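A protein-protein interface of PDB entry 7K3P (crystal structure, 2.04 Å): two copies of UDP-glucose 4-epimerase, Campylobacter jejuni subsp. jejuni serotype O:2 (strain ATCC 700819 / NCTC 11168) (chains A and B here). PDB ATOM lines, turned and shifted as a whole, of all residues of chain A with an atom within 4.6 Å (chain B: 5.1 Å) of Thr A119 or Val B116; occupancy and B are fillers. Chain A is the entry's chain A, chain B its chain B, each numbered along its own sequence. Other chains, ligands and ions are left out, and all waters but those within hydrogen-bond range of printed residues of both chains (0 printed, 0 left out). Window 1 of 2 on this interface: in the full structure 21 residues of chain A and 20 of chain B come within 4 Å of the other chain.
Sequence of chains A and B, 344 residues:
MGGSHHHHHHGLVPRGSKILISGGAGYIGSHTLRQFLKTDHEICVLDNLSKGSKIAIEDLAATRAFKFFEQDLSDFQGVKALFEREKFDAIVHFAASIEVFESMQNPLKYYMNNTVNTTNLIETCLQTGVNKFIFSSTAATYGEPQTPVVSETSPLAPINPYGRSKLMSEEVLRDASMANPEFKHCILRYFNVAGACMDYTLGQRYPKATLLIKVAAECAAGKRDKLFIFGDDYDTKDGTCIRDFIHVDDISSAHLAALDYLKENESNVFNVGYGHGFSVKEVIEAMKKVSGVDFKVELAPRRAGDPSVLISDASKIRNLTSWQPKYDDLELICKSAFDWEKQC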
ATOM      1  N   PHE A  76      21.914   5.666   8.373  1.00  0.00           N
ATOM      2  CA  PHE A  76      21.210   6.253   7.231  1.00  0.00           C
ATOM      3  C   PHE A  76      21.491   7.748   7.087  1.00  0.00           C
ATOM      4  O   PHE A  76      21.579   8.263   5.965  1.00  0.00           O
ATOM      5  CB  PHE A  76      19.694   6.017   7.282  1.00  0.00           C
ATOM      6  CG  PHE A  76      19.277   4.567   7.128  1.00  0.00           C
ATOM      7  CD1 PHE A  76      20.201   3.583   6.797  1.00  0.00           C
ATOM      8  CD2 PHE A  76      17.940   4.199   7.329  1.00  0.00           C
ATOM      9  CE1 PHE A  76      19.805   2.231   6.672  1.00  0.00           C
ATOM     10  CE2 PHE A  76      17.534   2.857   7.199  1.00  0.00           C
ATOM     11  CZ  PHE A  76      18.472   1.878   6.873  1.00  0.00           C
ATOM     12  N   THR A 115      18.962  -6.016   2.035  1.00  0.00           N
ATOM     13  CA  THR A 115      17.735  -5.343   1.604  1.00  0.00           C
ATOM     14  C   THR A 115      17.483  -3.975   2.255  1.00  0.00           C
ATOM     15  O   THR A 115      17.128  -3.001   1.578  1.00  0.00           O
ATOM     16  CB  THR A 115      16.523  -6.237   1.876  1.00  0.00           C
ATOM     17  OG1 THR A 115      16.813  -7.573   1.416  1.00  0.00           O
ATOM     18  CG2 THR A 115      15.303  -5.701   1.183  1.00  0.00           C
ATOM     19  N   VAL A 116      17.635  -3.901   3.572  1.00  0.00           N
ATOM     20  CA  VAL A 116      17.363  -2.649   4.277  1.00  0.00           C
ATOM     21  C   VAL A 116      18.378  -1.562   3.918  1.00  0.00           C
ATOM     22  O   VAL A 116      17.994  -0.453   3.566  1.00  0.00           O
ATOM     23  CB  VAL A 116      17.292  -2.858   5.806  1.00  0.00           C
ATOM     24  CG1 VAL A 116      17.390  -1.526   6.542  1.00  0.00           C
ATOM     25  CG2 VAL A 116      15.994  -3.569   6.176  1.00  0.00           C
ATOM     26  N   ASN A 117      19.663  -1.875   4.020  1.00  0.00           N
ATOM     27  CA  ASN A 117      20.693  -0.886   3.717  1.00  0.00           C
ATOM     28  C   ASN A 117      20.597  -0.442   2.271  1.00  0.00           C
ATOM     29  O   ASN A 117      20.800   0.736   1.947  1.00  0.00           O
ATOM     30  CB  ASN A 117      22.095  -1.439   4.006  1.00  0.00           C
ATOM     31  CG  ASN A 117      22.406  -1.464   5.489  1.00  0.00           C
ATOM     32  OD1 ASN A 117      21.671  -0.881   6.263  1.00  0.00           O
ATOM     33  ND2 ASN A 117      23.485  -2.141   5.886  1.00  0.00           N
ATOM     34  N   THR A 118      20.285  -1.391   1.398  1.00  0.00           N
ATOM     35  CA  THR A 118      20.174  -1.070  -0.025  1.00  0.00           C
ATOM     36  C   THR A 118      18.979  -0.175  -0.276  1.00  0.00           C
ATOM     37  O   THR A 118      19.036   0.735  -1.102  1.00  0.00           O
ATOM     38  CB  THR A 118      20.130  -2.349  -0.900  1.00  0.00           C
ATOM     39  OG1 THR A 118      21.374  -3.045  -0.754  1.00  0.00           O
ATOM     40  CG2 THR A 118      19.942  -1.980  -2.377  1.00  0.00           C
ATOM     41  N   THR A 119      17.889  -0.408   0.452  1.00  0.00           N
ATOM     42  CA  THR A 119      16.699   0.415   0.271  1.00  0.00           C
ATOM     43  C   THR A 119      16.973   1.877   0.648  1.00  0.00           C
ATOM     44  O   THR A 119      16.607   2.808  -0.087  1.00  0.00           O
ATOM     45  CB  THR A 119      15.497  -0.128   1.075  1.00  0.00           C
ATOM     46  OG1 THR A 119      15.241  -1.472   0.662  1.00  0.00           O
ATOM     47  CG2 THR A 119      14.264   0.719   0.842  1.00  0.00           C
ATOM     48  N   ASN A 120      17.600   2.099   1.794  1.00  0.00           N
ATOM     49  CA  ASN A 120      17.933   3.475   2.148  1.00  0.00           C
ATOM     50  C   ASN A 120      18.864   4.100   1.101  1.00  0.00           C
ATOM     51  O   ASN A 120      18.727   5.270   0.748  1.00  0.00           O
ATOM     52  CB  ASN A 120      18.603   3.546   3.508  1.00  0.00           C
ATOM     53  CG  ASN A 120      19.092   4.946   3.809  1.00  0.00           C
ATOM     54  OD1 ASN A 120      18.283   5.850   4.005  1.00  0.00           O
ATOM     55  ND2 ASN A 120      20.410   5.141   3.795  1.00  0.00           N
ATOM     56  N   LEU A 121      19.825   3.311   0.627  1.00  0.00           N
ATOM     57  CA  LEU A 121      20.775   3.769  -0.385  1.00  0.00           C
ATOM     58  C   LEU A 121      20.045   4.243  -1.635  1.00  0.00           C
ATOM     59  O   LEU A 121      20.356   5.301  -2.186  1.00  0.00           O
ATOM     60  CB  LEU A 121      21.754   2.645  -0.717  1.00  0.00           C
ATOM     61  CG  LEU A 121      23.082   2.955  -1.394  1.00  0.00           C
ATOM     62  CD1 LEU A 121      23.832   4.072  -0.688  1.00  0.00           C
ATOM     63  CD2 LEU A 121      23.939   1.687  -1.421  1.00  0.00           C
ATOM     64  N   ILE A 122      19.068   3.466  -2.085  1.00  0.00           N
ATOM     65  CA  ILE A 122      18.291   3.850  -3.263  1.00  0.00           C
ATOM     66  C   ILE A 122      17.495   5.125  -3.023  1.00  0.00           C
ATOM     67  O   ILE A 122      17.500   6.037  -3.872  1.00  0.00           O
ATOM     68  CB  ILE A 122      17.359   2.716  -3.728  1.00  0.00           C
ATOM     69  CG1 ILE A 122      18.191   1.530  -4.231  1.00  0.00           C
ATOM     70  CG2 ILE A 122      16.401   3.210  -4.823  1.00  0.00           C
ATOM     71  CD1 ILE A 122      17.395   0.186  -4.259  1.00  0.00           C
ATOM     72  N   GLU A 123      16.806   5.206  -1.882  1.00  0.00           N
ATOM     73  CA  GLU A 123      16.071   6.434  -1.573  1.00  0.00           C
ATOM     74  C   GLU A 123      16.997   7.648  -1.602  1.00  0.00           C
ATOM     75  O   GLU A 123      16.637   8.698  -2.135  1.00  0.00           O
ATOM     76  CB  GLU A 123      15.362   6.363  -0.220  1.00  0.00           C
ATOM     77  CG  GLU A 123      14.576   7.648   0.071  1.00  0.00           C
ATOM     78  CD  GLU A 123      13.785   7.570   1.362  1.00  0.00           C
ATOM     79  OE1 GLU A 123      14.416   7.494   2.436  1.00  0.00           O
ATOM     80  OE2 GLU A 123      12.537   7.581   1.292  1.00  0.00           O
ATOM     81  N   VAL A 172      12.959  -3.267  -5.665  1.00  0.00           N
ATOM     82  CA  VAL A 172      12.946  -1.858  -5.260  1.00  0.00           C
ATOM     83  C   VAL A 172      13.565  -1.004  -6.374  1.00  0.00           C
ATOM     84  O   VAL A 172      13.034   0.052  -6.723  1.00  0.00           O
ATOM     85  CB  VAL A 172      13.669  -1.633  -3.917  1.00  0.00           C
ATOM     86  CG1 VAL A 172      13.695  -0.125  -3.545  1.00  0.00           C
ATOM     87  CG2 VAL A 172      12.980  -2.431  -2.798  1.00  0.00           C
ATOM     88  N   PHE B  76      15.689   2.797  14.879  1.00  0.00           N
ATOM     89  CA  PHE B  76      15.941   1.409  15.260  1.00  0.00           C
ATOM     90  C   PHE B  76      16.491   1.279  16.698  1.00  0.00           C
ATOM     91  O   PHE B  76      16.106   0.374  17.437  1.00  0.00           O
ATOM     92  CB  PHE B  76      16.890   0.700  14.272  1.00  0.00           C
ATOM     93  CG  PHE B  76      16.365   0.619  12.836  1.00  0.00           C
ATOM     94  CD1 PHE B  76      15.051   0.950  12.539  1.00  0.00           C
ATOM     95  CD2 PHE B  76      17.200   0.209  11.802  1.00  0.00           C
ATOM     96  CE1 PHE B  76      14.568   0.893  11.222  1.00  0.00           C
ATOM     97  CE2 PHE B  76      16.728   0.140  10.489  1.00  0.00           C
ATOM     98  CZ  PHE B  76      15.403   0.491  10.204  1.00  0.00           C
ATOM     99  N   LEU B 108       9.669   4.395  -2.652  1.00  0.00           N
ATOM    100  CA  LEU B 108      10.628   4.321  -1.555  1.00  0.00           C
ATOM    101  C   LEU B 108      10.005   4.654  -0.191  1.00  0.00           C
ATOM    102  O   LEU B 108      10.379   4.046   0.817  1.00  0.00           O
ATOM    103  CB  LEU B 108      11.897   5.126  -1.840  1.00  0.00           C
ATOM    104  CG  LEU B 108      12.944   4.329  -2.638  1.00  0.00           C
ATOM    105  CD1 LEU B 108      13.475   3.136  -1.839  1.00  0.00           C
ATOM    106  CD2 LEU B 108      12.355   3.819  -3.953  1.00  0.00           C
ATOM    107  N   TYR B 111       8.618   1.203   0.766  1.00  0.00           N
ATOM    108  CA  TYR B 111       9.658   0.244   1.147  1.00  0.00           C
ATOM    109  C   TYR B 111      10.355   0.640   2.450  1.00  0.00           C
ATOM    110  O   TYR B 111      10.780  -0.227   3.220  1.00  0.00           O
ATOM    111  CB  TYR B 111      10.678   0.034   0.016  1.00  0.00           C
ATOM    112  CG  TYR B 111      10.081  -0.697  -1.167  1.00  0.00           C
ATOM    113  CD1 TYR B 111       9.582  -1.997  -1.023  1.00  0.00           C
ATOM    114  CD2 TYR B 111       9.999  -0.087  -2.419  1.00  0.00           C
ATOM    115  CE1 TYR B 111       9.026  -2.670  -2.099  1.00  0.00           C
ATOM    116  CE2 TYR B 111       9.454  -0.749  -3.505  1.00  0.00           C
ATOM    117  CZ  TYR B 111       8.964  -2.039  -3.334  1.00  0.00           C
ATOM    118  OH  TYR B 111       8.413  -2.698  -4.396  1.00  0.00           O
ATOM    119  N   MET B 112      10.487   1.943   2.696  1.00  0.00           N
ATOM    120  CA  MET B 112      11.108   2.398   3.943  1.00  0.00           C
ATOM    121  C   MET B 112      10.150   2.259   5.120  1.00  0.00           C
ATOM    122  O   MET B 112      10.493   1.674   6.139  1.00  0.00           O
ATOM    123  CB  MET B 112      11.577   3.863   3.837  1.00  0.00           C
ATOM    124  CG  MET B 112      12.766   4.062   2.908  1.00  0.00           C
ATOM    125  SD  MET B 112      14.300   3.289   3.442  1.00  0.00           S
ATOM    126  CE  MET B 112      14.748   4.379   4.816  1.00  0.00           C
ATOM    127  N   ASN B 114       7.313   0.637   5.411  1.00  0.00           N
ATOM    128  CA  ASN B 114       6.730  -0.686   5.610  1.00  0.00           C
ATOM    129  C   ASN B 114       7.796  -1.756   5.763  1.00  0.00           C
ATOM    130  O   ASN B 114       8.071  -2.215   6.868  1.00  0.00           O
ATOM    131  CB  ASN B 114       5.770  -1.025   4.459  1.00  0.00           C
ATOM    132  CG  ASN B 114       4.553  -0.128   4.440  1.00  0.00           C
ATOM    133  OD1 ASN B 114       4.391   0.731   5.307  1.00  0.00           O
ATOM    134  ND2 ASN B 114       3.689  -0.313   3.445  1.00  0.00           N
ATOM    135  N   THR B 115       8.425  -2.135   4.654  1.00  0.00           N
ATOM    136  CA  THR B 115       9.390  -3.238   4.667  1.00  0.00           C
ATOM    137  C   THR B 115      10.588  -3.038   5.587  1.00  0.00           C
ATOM    138  O   THR B 115      10.941  -3.926   6.398  1.00  0.00           O
ATOM    139  CB  THR B 115       9.905  -3.494   3.238  1.00  0.00           C
ATOM    140  OG1 THR B 115       8.780  -3.463   2.348  1.00  0.00           O
ATOM    141  CG2 THR B 115      10.619  -4.846   3.155  1.00  0.00           C
ATOM    142  N   VAL B 116      11.239  -1.888   5.454  1.00  0.00           N
ATOM    143  CA  VAL B 116      12.421  -1.616   6.247  1.00  0.00           C
ATOM    144  C   VAL B 116      12.089  -1.517   7.747  1.00  0.00           C
ATOM    145  O   VAL B 116      12.770  -2.142   8.574  1.00  0.00           O
ATOM    146  CB  VAL B 116      13.163  -0.340   5.751  1.00  0.00           C
ATOM    147  CG1 VAL B 116      14.219   0.108   6.770  1.00  0.00           C
ATOM    148  CG2 VAL B 116      13.825  -0.591   4.384  1.00  0.00           C
ATOM    149  N   ASN B 117      11.085  -0.719   8.108  1.00  0.00           N
ATOM    150  CA  ASN B 117      10.739  -0.593   9.533  1.00  0.00           C
ATOM    151  C   ASN B 117      10.320  -1.935  10.119  1.00  0.00           C
ATOM    152  O   ASN B 117      10.710  -2.278  11.241  1.00  0.00           O
ATOM    153  CB  ASN B 117       9.651   0.463   9.773  1.00  0.00           C
ATOM    154  CG  ASN B 117      10.184   1.889   9.654  1.00  0.00           C
ATOM    155  OD1 ASN B 117      11.391   2.099   9.617  1.00  0.00           O
ATOM    156  ND2 ASN B 117       9.279   2.865   9.571  1.00  0.00           N
ATOM    157  N   THR B 118       9.524  -2.689   9.360  1.00  0.00           N
ATOM    158  CA  THR B 118       9.080  -4.011   9.811  1.00  0.00           C
ATOM    159  C   THR B 118      10.257  -4.967   9.985  1.00  0.00           C
ATOM    160  O   THR B 118      10.292  -5.758  10.938  1.00  0.00           O
ATOM    161  CB  THR B 118       8.029  -4.617   8.877  1.00  0.00           C
ATOM    162  OG1 THR B 118       6.913  -3.728   8.788  1.00  0.00           O
ATOM    163  CG2 THR B 118       7.532  -5.961   9.421  1.00  0.00           C
ATOM    164  N   THR B 119      11.225  -4.901   9.073  1.00  0.00           N
ATOM    165  CA  THR B 119      12.402  -5.768   9.172  1.00  0.00           C
ATOM    166  C   THR B 119      13.165  -5.540  10.497  1.00  0.00           C
ATOM    167  O   THR B 119      13.519  -6.499  11.215  1.00  0.00           O
ATOM    168  CB  THR B 119      13.333  -5.617   7.949  1.00  0.00           C
ATOM    169  OG1 THR B 119      12.588  -5.886   6.745  1.00  0.00           O
ATOM    170  CG2 THR B 119      14.489  -6.586   8.035  1.00  0.00           C
ATOM    171  N   ASN B 120      13.421  -4.285  10.840  1.00  0.00           N
ATOM    172  CA  ASN B 120      14.092  -4.026  12.114  1.00  0.00           C
ATOM    173  C   ASN B 120      13.228  -4.492  13.297  1.00  0.00           C
ATOM    174  O   ASN B 120      13.742  -5.023  14.292  1.00  0.00           O
ATOM    175  CB  ASN B 120      14.427  -2.550  12.286  1.00  0.00           C
ATOM    176  CG  ASN B 120      14.924  -2.249  13.688  1.00  0.00           C
ATOM    177  OD1 ASN B 120      16.038  -2.614  14.041  1.00  0.00           O
ATOM    178  ND2 ASN B 120      14.075  -1.623  14.506  1.00  0.00           N
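The side-chain hydroxyl of Thr A119 sits at hydrogen-bond distance from the backbone carbonyl oxygen of Thr A115 (2.6 Å).
O of Tyr B111 sits at hydrogen-bond distance from N of Val B116.
O of Met B112 is in hydrogen-bond range of N of Asn B117.
The side-chain hydroxyl of Thr B119 lies within hydrogen-bond range of the backbone carbonyl oxygen of Thr B115.
CE2 of Phe A76 touches CE of Met B112, at 3.97 Å.
Val A116 touches Val B116 (CG1 to CG1, 3.6 Å).
Thr B119 touches Val A116.
O of Thr A119 touches CD1 of Leu B108 (3.6 Å).
Tyr B111 touches Thr A119.
CB of Thr A119 touches CG2 of Val B116 (3.7 Å).
CA of Glu A123 touches CG of Leu B108 (3.9 Å).
OE1 of Glu A123 touches CG of Met B112, 3.8 Å away.
Leu B108 touches Val A172.
CG2 of Val A172 touches CG of Tyr B111 (3.8 Å).
Printed residues of chain B within 4 Å of Val A116: Val B116 (3.6 Å) and Thr B119 (3.8 Å).
Of the printed residues of chain B, Val A172 touches Leu B108 and Tyr B111.
Of chain A, only Val A116 (3.6 Å) and Thr A119 (3.7 Å) come within 4 Å of Val B116.
The nearest printed residue of chain B that does not touch Thr A119 is Thr B115 (6.2 Å).
The nearest residue of chain A that does not touch Val B116 is Phe A76 (4.3 Å).
The nearest printed residue of chain A that does not touch Thr B119 is Thr A115 (6.2 Å).
Printed residues of chain B that touch a printed residue of chain A: Leu B108, Tyr B111, Met B112, Val B116 and Thr B119.
Hydrophobic or aromatic side chains of chain B within 4 Å of the printed part of chain A: Leu B108, Tyr B111, Met B112 and Val B116.
Of the 11 printed residues of chain A, 6 touch a printed residue of chain B.
Printed residues of chain A that touch a printed residue of chain B: Phe A76, Val A116, Thr A119, Asn A120, Glu A123 and Val A172.
Hydrophobic or aromatic side chains of chain A that line the printed part of chain B: Phe A76, Val A116 and Val A172.
Among the printed residues, no Asp or Glu carboxylate lies within 4 Å of a Lys or Arg side-chain nitrogen of the other chain.
Val A116 touches its own counterpart, Val B116.
Val A116 touches Thr B119, and with the chains exchanged Thr A119 touches Val B116.
Of the 12 pairs that touch across the chains among the printed residues, 3 have their exchanged pair printed and touching as well.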
